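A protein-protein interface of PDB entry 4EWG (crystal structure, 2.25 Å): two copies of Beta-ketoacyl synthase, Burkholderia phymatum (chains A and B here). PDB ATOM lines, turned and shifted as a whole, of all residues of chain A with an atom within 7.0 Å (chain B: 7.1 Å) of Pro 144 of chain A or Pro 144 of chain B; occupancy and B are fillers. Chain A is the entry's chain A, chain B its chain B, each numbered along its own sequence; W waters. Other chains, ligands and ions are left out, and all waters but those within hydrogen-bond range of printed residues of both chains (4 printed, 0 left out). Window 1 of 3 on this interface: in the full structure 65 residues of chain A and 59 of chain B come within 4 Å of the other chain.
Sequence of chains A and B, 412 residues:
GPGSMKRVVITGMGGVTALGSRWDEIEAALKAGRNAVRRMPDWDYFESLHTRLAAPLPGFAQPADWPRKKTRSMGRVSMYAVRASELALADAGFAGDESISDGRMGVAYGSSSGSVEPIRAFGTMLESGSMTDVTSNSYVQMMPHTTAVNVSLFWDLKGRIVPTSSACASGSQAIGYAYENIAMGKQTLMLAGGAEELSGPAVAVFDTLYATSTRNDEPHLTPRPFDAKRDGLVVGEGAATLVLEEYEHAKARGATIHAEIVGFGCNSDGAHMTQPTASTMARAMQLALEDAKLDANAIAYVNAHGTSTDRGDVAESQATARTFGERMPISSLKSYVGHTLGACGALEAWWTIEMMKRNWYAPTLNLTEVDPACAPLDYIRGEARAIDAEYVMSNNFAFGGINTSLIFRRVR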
ATOM      1  N   TYR A 109      10.800 -30.732  19.562  1.00  0.00           N
ATOM      2  CA  TYR A 109      12.068 -31.305  19.098  1.00  0.00           C
ATOM      3  C   TYR A 109      13.071 -30.217  18.758  1.00  0.00           C
ATOM      4  O   TYR A 109      12.687 -29.110  18.365  1.00  0.00           O
ATOM      5  CB  TYR A 109      11.829 -32.133  17.809  1.00  0.00           C
ATOM      6  CG  TYR A 109      12.389 -33.507  17.835  1.00  0.00           C
ATOM      7  CD1 TYR A 109      13.743 -33.760  17.485  1.00  0.00           C
ATOM      8  CD2 TYR A 109      11.595 -34.590  18.216  1.00  0.00           C
ATOM      9  CE1 TYR A 109      14.264 -35.057  17.514  1.00  0.00           C
ATOM     10  CE2 TYR A 109      12.116 -35.891  18.237  1.00  0.00           C
ATOM     11  CZ  TYR A 109      13.437 -36.115  17.896  1.00  0.00           C
ATOM     12  OH  TYR A 109      13.927 -37.395  17.955  1.00  0.00           O
ATOM     13  N   GLY A 110      14.345 -30.563  18.846  1.00  0.00           N
ATOM     14  CA  GLY A 110      15.370 -29.676  18.355  1.00  0.00           C
ATOM     15  C   GLY A 110      16.730 -30.312  18.192  1.00  0.00           C
ATOM     16  O   GLY A 110      16.918 -31.500  18.475  1.00  0.00           O
ATOM     17  N   SER A 111      17.672 -29.496  17.724  1.00  0.00           N
ATOM     18  CA  SER A 111      19.038 -29.926  17.497  1.00  0.00           C
ATOM     19  C   SER A 111      19.935 -28.706  17.562  1.00  0.00           C
ATOM     20  O   SER A 111      19.447 -27.582  17.513  1.00  0.00           O
ATOM     21  CB  SER A 111      19.174 -30.602  16.117  1.00  0.00           C
ATOM     22  OG  SER A 111      18.773 -29.744  15.081  1.00  0.00           O
ATOM     23  N   SER A 112      21.234 -28.922  17.707  1.00  0.00           N
ATOM     24  CA  SER A 112      22.202 -27.816  17.788  1.00  0.00           C
ATOM     25  C   SER A 112      22.329 -27.142  16.430  1.00  0.00           C
ATOM     26  O   SER A 112      22.680 -25.957  16.337  1.00  0.00           O
ATOM     27  CB  SER A 112      23.609 -28.304  18.216  1.00  0.00           C
ATOM     28  OG  SER A 112      23.542 -29.131  19.365  1.00  0.00           O
ATOM     29  N   SER A 113      22.049 -27.906  15.383  1.00  0.00           N
ATOM     30  CA  SER A 113      22.291 -27.472  14.040  1.00  0.00           C
ATOM     31  C   SER A 113      21.433 -28.252  13.024  1.00  0.00           C
ATOM     32  O   SER A 113      20.953 -29.345  13.304  1.00  0.00           O
ATOM     33  CB  SER A 113      23.792 -27.694  13.768  1.00  0.00           C
ATOM     34  OG  SER A 113      24.103 -27.559  12.422  1.00  0.00           O
ATOM     35  N   GLY A 114      21.273 -27.665  11.837  1.00  0.00           N
ATOM     36  CA  GLY A 114      20.693 -28.317  10.710  1.00  0.00           C
ATOM     37  C   GLY A 114      21.687 -29.247  10.049  1.00  0.00           C
ATOM     38  O   GLY A 114      22.670 -29.675  10.675  1.00  0.00           O
ATOM     39  N   TYR A 139      16.708 -24.934   2.659  1.00  0.00           N
ATOM     40  CA  TYR A 139      16.329 -24.274   3.921  1.00  0.00           C
ATOM     41  C   TYR A 139      15.701 -25.261   4.895  1.00  0.00           C
ATOM     42  O   TYR A 139      16.058 -25.257   6.088  1.00  0.00           O
ATOM     43  CB  TYR A 139      15.388 -23.054   3.726  1.00  0.00           C
ATOM     44  CG  TYR A 139      15.016 -22.450   5.070  1.00  0.00           C
ATOM     45  CD1 TYR A 139      15.992 -21.844   5.867  1.00  0.00           C
ATOM     46  CD2 TYR A 139      13.739 -22.540   5.562  1.00  0.00           C
ATOM     47  CE1 TYR A 139      15.678 -21.297   7.100  1.00  0.00           C
ATOM     48  CE2 TYR A 139      13.407 -22.014   6.810  1.00  0.00           C
ATOM     49  CZ  TYR A 139      14.385 -21.405   7.591  1.00  0.00           C
ATOM     50  OH  TYR A 139      14.079 -20.888   8.849  1.00  0.00           O
ATOM     51  N   VAL A 140      14.787 -26.104   4.406  1.00  0.00           N
ATOM     52  CA  VAL A 140      14.051 -27.017   5.302  1.00  0.00           C
ATOM     53  C   VAL A 140      14.946 -28.095   5.922  1.00  0.00           C
ATOM     54  O   VAL A 140      14.700 -28.573   7.049  1.00  0.00           O
ATOM     55  CB  VAL A 140      12.821 -27.687   4.599  1.00  0.00           C
ATOM     56  CG1 VAL A 140      13.214 -28.502   3.361  1.00  0.00           C
ATOM     57  CG2 VAL A 140      12.082 -28.573   5.586  1.00  0.00           C
ATOM     58  N   GLN A 141      16.011 -28.446   5.216  1.00  0.00           N
ATOM     59  CA  GLN A 141      17.052 -29.343   5.790  1.00  0.00           C
ATOM     60  C   GLN A 141      18.023 -28.611   6.759  1.00  0.00           C
ATOM     61  O   GLN A 141      18.610 -29.232   7.640  1.00  0.00           O
ATOM     62  CB  GLN A 141      17.863 -29.987   4.667  1.00  0.00           C
ATOM     63  CG  GLN A 141      17.056 -30.865   3.730  1.00  0.00           C
ATOM     64  CD  GLN A 141      17.925 -31.606   2.707  1.00  0.00           C
ATOM     65  OE1 GLN A 141      19.169 -31.531   2.733  1.00  0.00           O
ATOM     66  NE2 GLN A 141      17.262 -32.370   1.816  1.00  0.00           N
ATOM     67  N   MET A 142      18.210 -27.310   6.553  1.00  0.00           N
ATOM     68  CA  MET A 142      19.114 -26.473   7.391  1.00  0.00           C
ATOM     69  C   MET A 142      18.412 -25.813   8.580  1.00  0.00           C
ATOM     70  O   MET A 142      19.016 -25.571   9.600  1.00  0.00           O
ATOM     71  CB  MET A 142      19.704 -25.337   6.567  1.00  0.00           C
ATOM     72  CG  MET A 142      20.782 -24.556   7.333  1.00  0.00           C
ATOM     73  SD  MET A 142      21.488 -23.206   6.410  1.00  0.00           S
ATOM     74  CE  MET A 142      22.193 -22.138   7.692  1.00  0.00           C
ATOM     75  N   MET A 143      17.111 -25.562   8.448  1.00  0.00           N
ATOM     76  CA  MET A 143      16.452 -24.659   9.378  1.00  0.00           C
ATOM     77  C   MET A 143      16.545 -25.129  10.866  1.00  0.00           C
ATOM     78  O   MET A 143      16.650 -26.296  11.151  1.00  0.00           O
ATOM     79  CB  MET A 143      15.017 -24.414   8.974  1.00  0.00           C
ATOM     80  CG  MET A 143      14.088 -25.638   9.048  1.00  0.00           C
ATOM     81  SD  MET A 143      12.587 -25.269   8.145  1.00  0.00           S
ATOM     82  CE  MET A 143      11.502 -26.505   8.827  1.00  0.00           C
ATOM     83  N   PRO A 144      16.531 -24.183  11.807  1.00  0.00           N
ATOM     84  CA  PRO A 144      16.609 -24.501  13.235  1.00  0.00           C
ATOM     85  C   PRO A 144      15.665 -25.630  13.637  1.00  0.00           C
ATOM     86  O   PRO A 144      16.008 -26.502  14.424  1.00  0.00           O
ATOM     87  CB  PRO A 144      16.177 -23.188  13.874  1.00  0.00           C
ATOM     88  CG  PRO A 144      16.719 -22.171  12.904  1.00  0.00           C
ATOM     89  CD  PRO A 144      16.377 -22.738  11.576  1.00  0.00           C
ATOM     90  N   HIS A 145      14.464 -25.575  13.090  1.00  0.00           N
ATOM     91  CA  HIS A 145      13.405 -26.496  13.452  1.00  0.00           C
ATOM     92  C   HIS A 145      13.218 -27.623  12.456  1.00  0.00           C
ATOM     93  O   HIS A 145      12.146 -28.179  12.375  1.00  0.00           O
ATOM     94  CB  HIS A 145      12.091 -25.737  13.701  1.00  0.00           C
ATOM     95  CG  HIS A 145      11.651 -24.839  12.555  1.00  0.00           C
ATOM     96  ND1 HIS A 145      12.504 -24.070  11.862  1.00  0.00           N
ATOM     97  CD2 HIS A 145      10.395 -24.598  12.020  1.00  0.00           C
ATOM     98  CE1 HIS A 145      11.821 -23.356  10.925  1.00  0.00           C
ATOM     99  NE2 HIS A 145      10.539 -23.689  11.007  1.00  0.00           N
ATOM    100  N   THR A 146      14.295 -28.001  11.741  1.00  0.00           N
ATOM    101  CA  THR A 146      14.247 -29.082  10.761  1.00  0.00           C
ATOM    102  C   THR A 146      13.785 -30.413  11.376  1.00  0.00           C
ATOM    103  O   THR A 146      12.937 -31.120  10.792  1.00  0.00           O
ATOM    104  CB  THR A 146      15.587 -29.266  10.014  1.00  0.00           C
ATOM    105  OG1 THR A 146      15.402 -30.158   8.908  1.00  0.00           O
ATOM    106  CG2 THR A 146      16.710 -29.757  10.933  1.00  0.00           C
ATOM    107  N   THR A 147      14.322 -30.751  12.549  1.00  0.00           N
ATOM    108  CA  THR A 147      13.935 -31.982  13.181  1.00  0.00           C
ATOM    109  C   THR A 147      12.409 -31.945  13.498  1.00  0.00           C
ATOM    110  O   THR A 147      11.683 -32.848  13.116  1.00  0.00           O
ATOM    111  CB  THR A 147      14.754 -32.278  14.442  1.00  0.00           C
ATOM    112  OG1 THR A 147      14.646 -31.187  15.347  1.00  0.00           O
ATOM    113  CG2 THR A 147      16.201 -32.543  14.102  1.00  0.00           C
ATOM    114  N   ALA A 148      11.942 -30.878  14.155  1.00  0.00           N
ATOM    115  CA  ALA A 148      10.561 -30.810  14.651  1.00  0.00           C
ATOM    116  C   ALA A 148       9.553 -30.863  13.503  1.00  0.00           C
ATOM    117  O   ALA A 148       8.531 -31.576  13.591  1.00  0.00           O
ATOM    118  CB  ALA A 148      10.318 -29.528  15.474  1.00  0.00           C
ATOM    119  N   PRO A 163       9.401 -25.822  19.031  1.00  0.00           N
ATOM    120  CA  PRO A 163      10.785 -25.998  18.578  1.00  0.00           C
ATOM    121  C   PRO A 163      11.649 -25.819  19.786  1.00  0.00           C
ATOM    122  O   PRO A 163      11.480 -24.823  20.480  1.00  0.00           O
ATOM    123  CB  PRO A 163      10.948 -24.883  17.514  1.00  0.00           C
ATOM    124  CG  PRO A 163       9.996 -23.829  17.940  1.00  0.00           C
ATOM    125  CD  PRO A 163       8.884 -24.472  18.734  1.00  0.00           C
ATOM    126  N   THR A 164      12.440 -26.820  20.153  1.00  0.00           N
ATOM    127  CA  THR A 164      13.347 -26.685  21.299  1.00  0.00           C
ATOM    128  C   THR A 164      14.786 -26.862  20.852  1.00  0.00           C
ATOM    129  O   THR A 164      15.516 -27.678  21.372  1.00  0.00           O
ATOM    130  CB  THR A 164      12.983 -27.715  22.361  1.00  0.00           C
ATOM    131  OG1 THR A 164      13.059 -29.027  21.794  1.00  0.00           O
ATOM    132  CG2 THR A 164      11.550 -27.458  22.852  1.00  0.00           C
ATOM    133  N   SER A 165      15.186 -26.113  19.840  1.00  0.00           N
ATOM    134  CA  SER A 165      16.585 -26.188  19.372  1.00  0.00           C
ATOM    135  C   SER A 165      17.466 -25.296  20.235  1.00  0.00           C
ATOM    136  O   SER A 165      17.557 -24.070  20.014  1.00  0.00           O
ATOM    137  CB  SER A 165      16.707 -25.859  17.898  1.00  0.00           C
ATOM    138  OG  SER A 165      16.257 -26.941  17.117  1.00  0.00           O
ATOM    139  N   SER A 166      18.080 -25.915  21.254  1.00  0.00           N
ATOM    140  CA  SER A 166      18.876 -25.171  22.267  1.00  0.00           C
ATOM    141  C   SER A 166      20.166 -25.920  22.546  1.00  0.00           C
ATOM    142  O   SER A 166      20.558 -26.142  23.698  1.00  0.00           O
ATOM    143  CB  SER A 166      18.057 -25.004  23.542  1.00  0.00           C
ATOM    144  OG  SER A 166      17.447 -26.219  23.962  1.00  0.00           O
ATOM    145  N   ALA A 167      20.835 -26.299  21.479  1.00  0.00           N
ATOM    146  CA  ALA A 167      22.060 -27.077  21.558  1.00  0.00           C
ATOM    147  C   ALA A 167      21.850 -28.298  22.451  1.00  0.00           C
ATOM    148  O   ALA A 167      20.893 -29.082  22.228  1.00  0.00           O
ATOM    149  CB  ALA A 167      23.191 -26.200  22.049  1.00  0.00           C
ATOM    150  N   TYR B 109      12.334 -16.254  22.262  1.00  0.00           N
ATOM    151  CA  TYR B 109      12.780 -15.588  21.050  1.00  0.00           C
ATOM    152  C   TYR B 109      13.227 -16.568  20.006  1.00  0.00           C
ATOM    153  O   TYR B 109      13.693 -17.690  20.329  1.00  0.00           O
ATOM    154  CB  TYR B 109      13.971 -14.706  21.389  1.00  0.00           C
ATOM    155  CG  TYR B 109      13.850 -13.275  20.945  1.00  0.00           C
ATOM    156  CD1 TYR B 109      14.232 -12.893  19.687  1.00  0.00           C
ATOM    157  CD2 TYR B 109      13.351 -12.304  21.814  1.00  0.00           C
ATOM    158  CE1 TYR B 109      14.120 -11.574  19.272  1.00  0.00           C
ATOM    159  CE2 TYR B 109      13.244 -10.975  21.429  1.00  0.00           C
ATOM    160  CZ  TYR B 109      13.638 -10.619  20.142  1.00  0.00           C
ATOM    161  OH  TYR B 109      13.515  -9.332  19.735  1.00  0.00           O
ATOM    162  N   GLY B 110      13.151 -16.156  18.743  1.00  0.00           N
ATOM    163  CA  GLY B 110      13.768 -16.932  17.689  1.00  0.00           C
ATOM    164  C   GLY B 110      13.954 -16.193  16.403  1.00  0.00           C
ATOM    165  O   GLY B 110      13.551 -15.039  16.269  1.00  0.00           O
ATOM    166  N   SER B 111      14.513 -16.901  15.420  1.00  0.00           N
ATOM    167  CA  SER B 111      14.728 -16.353  14.083  1.00  0.00           C
ATOM    168  C   SER B 111      14.752 -17.479  13.075  1.00  0.00           C
ATOM    169  O   SER B 111      14.876 -18.647  13.460  1.00  0.00           O
ATOM    170  CB  SER B 111      16.058 -15.610  14.042  1.00  0.00           C
ATOM    171  OG  SER B 111      17.140 -16.454  14.379  1.00  0.00           O
ATOM    172  N   SER B 112      14.614 -17.162  11.800  1.00  0.00           N
ATOM    173  CA  SER B 112      14.662 -18.221  10.746  1.00  0.00           C
ATOM    174  C   SER B 112      16.060 -18.825  10.627  1.00  0.00           C
ATOM    175  O   SER B 112      16.239 -19.943  10.179  1.00  0.00           O
ATOM    176  CB  SER B 112      14.245 -17.649   9.379  1.00  0.00           C
ATOM    177  OG  SER B 112      13.038 -16.922   9.493  1.00  0.00           O
ATOM    178  N   SER B 113      17.039 -18.029  11.005  1.00  0.00           N
ATOM    179  CA  SER B 113      18.396 -18.347  10.787  1.00  0.00           C
ATOM    180  C   SER B 113      19.309 -17.572  11.740  1.00  0.00           C
ATOM    181  O   SER B 113      18.952 -16.517  12.264  1.00  0.00           O
ATOM    182  CB  SER B 113      18.714 -18.007   9.318  1.00  0.00           C
ATOM    183  OG  SER B 113      20.105 -18.085   9.065  1.00  0.00           O
ATOM    184  N   GLY B 114      20.500 -18.094  11.947  1.00  0.00           N
ATOM    185  CA  GLY B 114      21.560 -17.350  12.630  1.00  0.00           C
ATOM    186  C   GLY B 114      22.193 -16.315  11.715  1.00  0.00           C
ATOM    187  O   GLY B 114      21.607 -15.942  10.712  1.00  0.00           O
ATOM    188  N   TYR B 139      29.802 -20.456  16.625  1.00  0.00           N
ATOM    189  CA  TYR B 139      28.590 -21.216  16.941  1.00  0.00           C
ATOM    190  C   TYR B 139      27.520 -20.358  17.613  1.00  0.00           C
ATOM    191  O   TYR B 139      26.343 -20.414  17.220  1.00  0.00           O
ATOM    192  CB  TYR B 139      28.862 -22.484  17.783  1.00  0.00           C
ATOM    193  CG  TYR B 139      27.543 -23.207  18.060  1.00  0.00           C
ATOM    194  CD1 TYR B 139      26.826 -23.809  17.019  1.00  0.00           C
ATOM    195  CD2 TYR B 139      26.974 -23.205  19.321  1.00  0.00           C
ATOM    196  CE1 TYR B 139      25.590 -24.409  17.247  1.00  0.00           C
ATOM    197  CE2 TYR B 139      25.767 -23.825  19.562  1.00  0.00           C
ATOM    198  CZ  TYR B 139      25.068 -24.428  18.521  1.00  0.00           C
ATOM    199  OH  TYR B 139      23.855 -25.016  18.750  1.00  0.00           O
ATOM    200  N   VAL B 140      27.905 -19.562  18.604  1.00  0.00           N
ATOM    201  CA  VAL B 140      26.905 -18.804  19.366  1.00  0.00           C
ATOM    202  C   VAL B 140      26.243 -17.692  18.511  1.00  0.00           C
ATOM    203  O   VAL B 140      25.103 -17.272  18.793  1.00  0.00           O
ATOM    204  CB  VAL B 140      27.434 -18.256  20.733  1.00  0.00           C
ATOM    205  CG1 VAL B 140      27.827 -19.428  21.659  1.00  0.00           C
ATOM    206  CG2 VAL B 140      28.582 -17.277  20.541  1.00  0.00           C
ATOM    207  N   GLN B 141      26.948 -17.236  17.474  1.00  0.00           N
ATOM    208  CA  GLN B 141      26.359 -16.312  16.492  1.00  0.00           C
ATOM    209  C   GLN B 141      25.454 -16.994  15.444  1.00  0.00           C
ATOM    210  O   GLN B 141      24.522 -16.378  14.912  1.00  0.00           O
ATOM    211  CB  GLN B 141      27.465 -15.539  15.771  1.00  0.00           C
ATOM    212  CG  GLN B 141      28.322 -14.689  16.690  1.00  0.00           C
ATOM    213  CD  GLN B 141      29.453 -13.986  15.933  1.00  0.00           C
ATOM    214  OE1 GLN B 141      29.392 -13.834  14.698  1.00  0.00           O
ATOM    215  NE2 GLN B 141      30.511 -13.604  16.656  1.00  0.00           N
ATOM    216  N   MET B 142      25.749 -18.257  15.172  1.00  0.00           N
ATOM    217  CA  MET B 142      24.982 -19.055  14.205  1.00  0.00           C
ATOM    218  C   MET B 142      23.807 -19.767  14.853  1.00  0.00           C
ATOM    219  O   MET B 142      22.842 -20.076  14.183  1.00  0.00           O
ATOM    220  CB  MET B 142      25.865 -20.118  13.566  1.00  0.00           C
ATOM    221  CG  MET B 142      25.173 -20.854  12.399  1.00  0.00           C
ATOM    222  SD  MET B 142      26.206 -22.089  11.651  1.00  0.00           S
ATOM    223  CE  MET B 142      25.025 -23.309  11.087  1.00  0.00           C
ATOM    224  N   MET B 143      23.908 -20.081  16.138  1.00  0.00           N
ATOM    225  CA  MET B 143      23.062 -21.114  16.682  1.00  0.00           C
ATOM    226  C   MET B 143      21.575 -20.786  16.552  1.00  0.00           C
ATOM    227  O   MET B 143      21.188 -19.632  16.530  1.00  0.00           O
ATOM    228  CB  MET B 143      23.466 -21.450  18.121  1.00  0.00           C
ATOM    229  CG  MET B 143      23.277 -20.353  19.149  1.00  0.00           C
ATOM    230  SD  MET B 143      24.168 -20.718  20.673  1.00  0.00           S
ATOM    231  CE  MET B 143      23.580 -19.330  21.653  1.00  0.00           C
ATOM    232  N   PRO B 144      20.732 -21.804  16.437  1.00  0.00           N
ATOM    233  CA  PRO B 144      19.278 -21.609  16.328  1.00  0.00           C
ATOM    234  C   PRO B 144      18.736 -20.626  17.332  1.00  0.00           C
ATOM    235  O   PRO B 144      17.884 -19.797  17.014  1.00  0.00           O
ATOM    236  CB  PRO B 144      18.735 -23.013  16.646  1.00  0.00           C
ATOM    237  CG  PRO B 144      19.805 -23.890  16.084  1.00  0.00           C
ATOM    238  CD  PRO B 144      21.073 -23.233  16.530  1.00  0.00           C
ATOM    239  N   HIS B 145      19.251 -20.717  18.542  1.00  0.00           N
ATOM    240  CA  HIS B 145      18.794 -19.870  19.648  1.00  0.00           C
ATOM    241  C   HIS B 145      19.671 -18.670  19.948  1.00  0.00           C
ATOM    242  O   HIS B 145      19.687 -18.184  21.071  1.00  0.00           O
ATOM    243  CB  HIS B 145      18.574 -20.731  20.918  1.00  0.00           C
ATOM    244  CG  HIS B 145      19.776 -21.566  21.346  1.00  0.00           C
ATOM    245  ND1 HIS B 145      20.515 -22.293  20.482  1.00  0.00           N
ATOM    246  CD2 HIS B 145      20.298 -21.833  22.618  1.00  0.00           C
ATOM    247  CE1 HIS B 145      21.486 -22.942  21.140  1.00  0.00           C
ATOM    248  NE2 HIS B 145      21.353 -22.673  22.452  1.00  0.00           N
ATOM    249  N   THR B 146      20.358 -18.155  18.940  1.00  0.00           N
ATOM    250  CA  THR B 146      21.290 -17.033  19.143  1.00  0.00           C
ATOM    251  C   THR B 146      20.588 -15.800  19.676  1.00  0.00           C
ATOM    252  O   THR B 146      21.066 -15.150  20.604  1.00  0.00           O
ATOM    253  CB  THR B 146      22.101 -16.692  17.867  1.00  0.00           C
ATOM    254  OG1 THR B 146      23.179 -15.824  18.202  1.00  0.00           O
ATOM    255  CG2 THR B 146      21.210 -16.027  16.789  1.00  0.00           C
ATOM    256  N   THR B 147      19.427 -15.505  19.124  1.00  0.00           N
ATOM    257  CA  THR B 147      18.669 -14.359  19.563  1.00  0.00           C
ATOM    258  C   THR B 147      18.265 -14.526  21.023  1.00  0.00           C
ATOM    259  O   THR B 147      18.545 -13.642  21.835  1.00  0.00           O
ATOM    260  CB  THR B 147      17.424 -14.100  18.679  1.00  0.00           C
ATOM    261  OG1 THR B 147      16.601 -15.266  18.640  1.00  0.00           O
ATOM    262  CG2 THR B 147      17.824 -13.740  17.229  1.00  0.00           C
ATOM    263  N   ALA B 148      17.664 -15.677  21.383  1.00  0.00           N
ATOM    264  CA  ALA B 148      17.112 -15.825  22.720  1.00  0.00           C
ATOM    265  C   ALA B 148      18.194 -15.741  23.780  1.00  0.00           C
ATOM    266  O   ALA B 148      18.001 -15.109  24.875  1.00  0.00           O
ATOM    267  CB  ALA B 148      16.353 -17.120  22.864  1.00  0.00           C
ATOM    268  N   PRO B 163      13.099 -21.286  23.185  1.00  0.00           N
ATOM    269  CA  PRO B 163      13.718 -20.958  21.890  1.00  0.00           C
ATOM    270  C   PRO B 163      12.846 -21.154  20.651  1.00  0.00           C
ATOM    271  O   PRO B 163      13.063 -22.103  19.855  1.00  0.00           O
ATOM    272  CB  PRO B 163      14.863 -21.950  21.782  1.00  0.00           C
ATOM    273  CG  PRO B 163      14.405 -23.132  22.566  1.00  0.00           C
ATOM    274  CD  PRO B 163      13.513 -22.618  23.678  1.00  0.00           C
ATOM    275  N   THR B 164      11.977 -20.203  20.421  1.00  0.00           N
ATOM    276  CA  THR B 164      10.968 -20.295  19.367  1.00  0.00           C
ATOM    277  C   THR B 164      11.473 -19.933  17.961  1.00  0.00           C
ATOM    278  O   THR B 164      10.914 -19.074  17.287  1.00  0.00           O
ATOM    279  CB  THR B 164       9.799 -19.394  19.761  1.00  0.00           C
ATOM    280  OG1 THR B 164      10.273 -18.021  19.865  1.00  0.00           O
ATOM    281  CG2 THR B 164       9.206 -19.886  21.081  1.00  0.00           C
ATOM    282  N   SER B 165      12.501 -20.611  17.494  1.00  0.00           N
ATOM    283  CA  SER B 165      13.003 -20.381  16.116  1.00  0.00           C
ATOM    284  C   SER B 165      12.236 -21.250  15.131  1.00  0.00           C
ATOM    285  O   SER B 165      12.586 -22.445  14.888  1.00  0.00           O
ATOM    286  CB  SER B 165      14.505 -20.622  16.005  1.00  0.00           C
ATOM    287  OG  SER B 165      15.206 -19.558  16.636  1.00  0.00           O
ATOM    288  N   SER B 166      11.194 -20.659  14.572  1.00  0.00           N
ATOM    289  CA  SER B 166      10.275 -21.388  13.683  1.00  0.00           C
ATOM    290  C   SER B 166       9.994 -20.597  12.412  1.00  0.00           C
ATOM    291  O   SER B 166       8.848 -20.414  12.006  1.00  0.00           O
ATOM    292  CB  SER B 166       8.980 -21.708  14.441  1.00  0.00           C
ATOM    293  OG  SER B 166       8.466 -20.565  15.122  1.00  0.00           O
ATOM    294  N   ALA B 167      11.049 -20.122  11.792  1.00  0.00           N
ATOM    295  CA  ALA B 167      10.964 -19.247  10.641  1.00  0.00           C
ATOM    296  C   ALA B 167       9.960 -18.088  10.936  1.00  0.00           C
ATOM    297  O   ALA B 167      10.098 -17.379  11.985  1.00  0.00           O
ATOM    298  CB  ALA B 167      10.622 -20.036   9.389  1.00  0.00           C
HETATM  299  O   HOH W   1      22.275 -24.082  24.680  1.00  0.00           O
HETATM  300  O   HOH W   2      13.694 -21.145  12.383  1.00  0.00           O
HETATM  301  O   HOH W   3      14.250 -24.334  16.619  1.00  0.00           O
HETATM  302  O   HOH W   4       8.361 -22.220  10.205  1.00  0.00           O
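The backbone carbonyl oxygen (O) of Ser 112 of chain A is in hydrogen-bond range of the side-chain hydroxyl (OH) of Tyr 139 of chain B (2.8 Å). The backbone carbonyl oxygen (O) of Ser 165 of chain A is in hydrogen-bond range of a ring nitrogen (ND1) of His 145 of chain B, 3.5 Å away. OH of Tyr 139 of chain A lies within hydrogen-bond range of O of Ser 112 of chain B, at 2.7 Å. The backbone carbonyl oxygen (O) of Pro 163 of chain A lies close to the backbone carbonyl oxygen (O) of Pro 163 of chain B, 3.2 Å away. A ring nitrogen (ND1) of His 145 of chain A sits at hydrogen-bond distance from the backbone carbonyl oxygen (O) of Ser 165 of chain B (3.4 Å).
The backbone carbonyl oxygen of Pro 144 of chain B lies within hydrogen-bond range of the side-chain hydroxyl of Ser 165 of chain B (2.7 Å).
Of chain A, only Ser 111, Ser 112, Pro 144 and Ser 165 come within 4 Å of Pro 144 of chain B. Of the printed residues of chain A, His 145 of chain B touches Ser 165 (3.5 Å), Ser 166 (3.5 Å) and Ala 167 (3.4 Å). Gly 110 of chain B touches none of the printed residues of chain A. The nearest residue of chain A that does not touch Pro 144 of chain B is Ser 113 of chain A (4.7 Å).
Hydrophobic or aromatic side chains of chain A that line the printed part of chain B: Tyr 139, Pro 144, His 145, Pro 163 and Ala 167. Of the 21 printed residues of chain B, 9 touch a printed residue of chain A. Along chain B the printed residues that touch a printed residue of chain A span positions 112 to 167. Among the printed residues, 21 pairs touch across the chains. Among the printed residues, no Asp or Glu carboxylate lies within 4 Å of a Lys or Arg side-chain nitrogen of the other chain.
His 145 of chain A touches Ser 166 of chain B, and with the chains exchanged Ser 166 of chain A touches His 145 of chain B. 21 positions are printed for both chains.
Water W3 lies within hydrogen-bond range of the backbone carbonyl oxygen (O) of Ser 165 of chain B (3.1 Å) and the side-chain hydroxyl (OG) of Ser 165 of chain A (3.3 Å).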
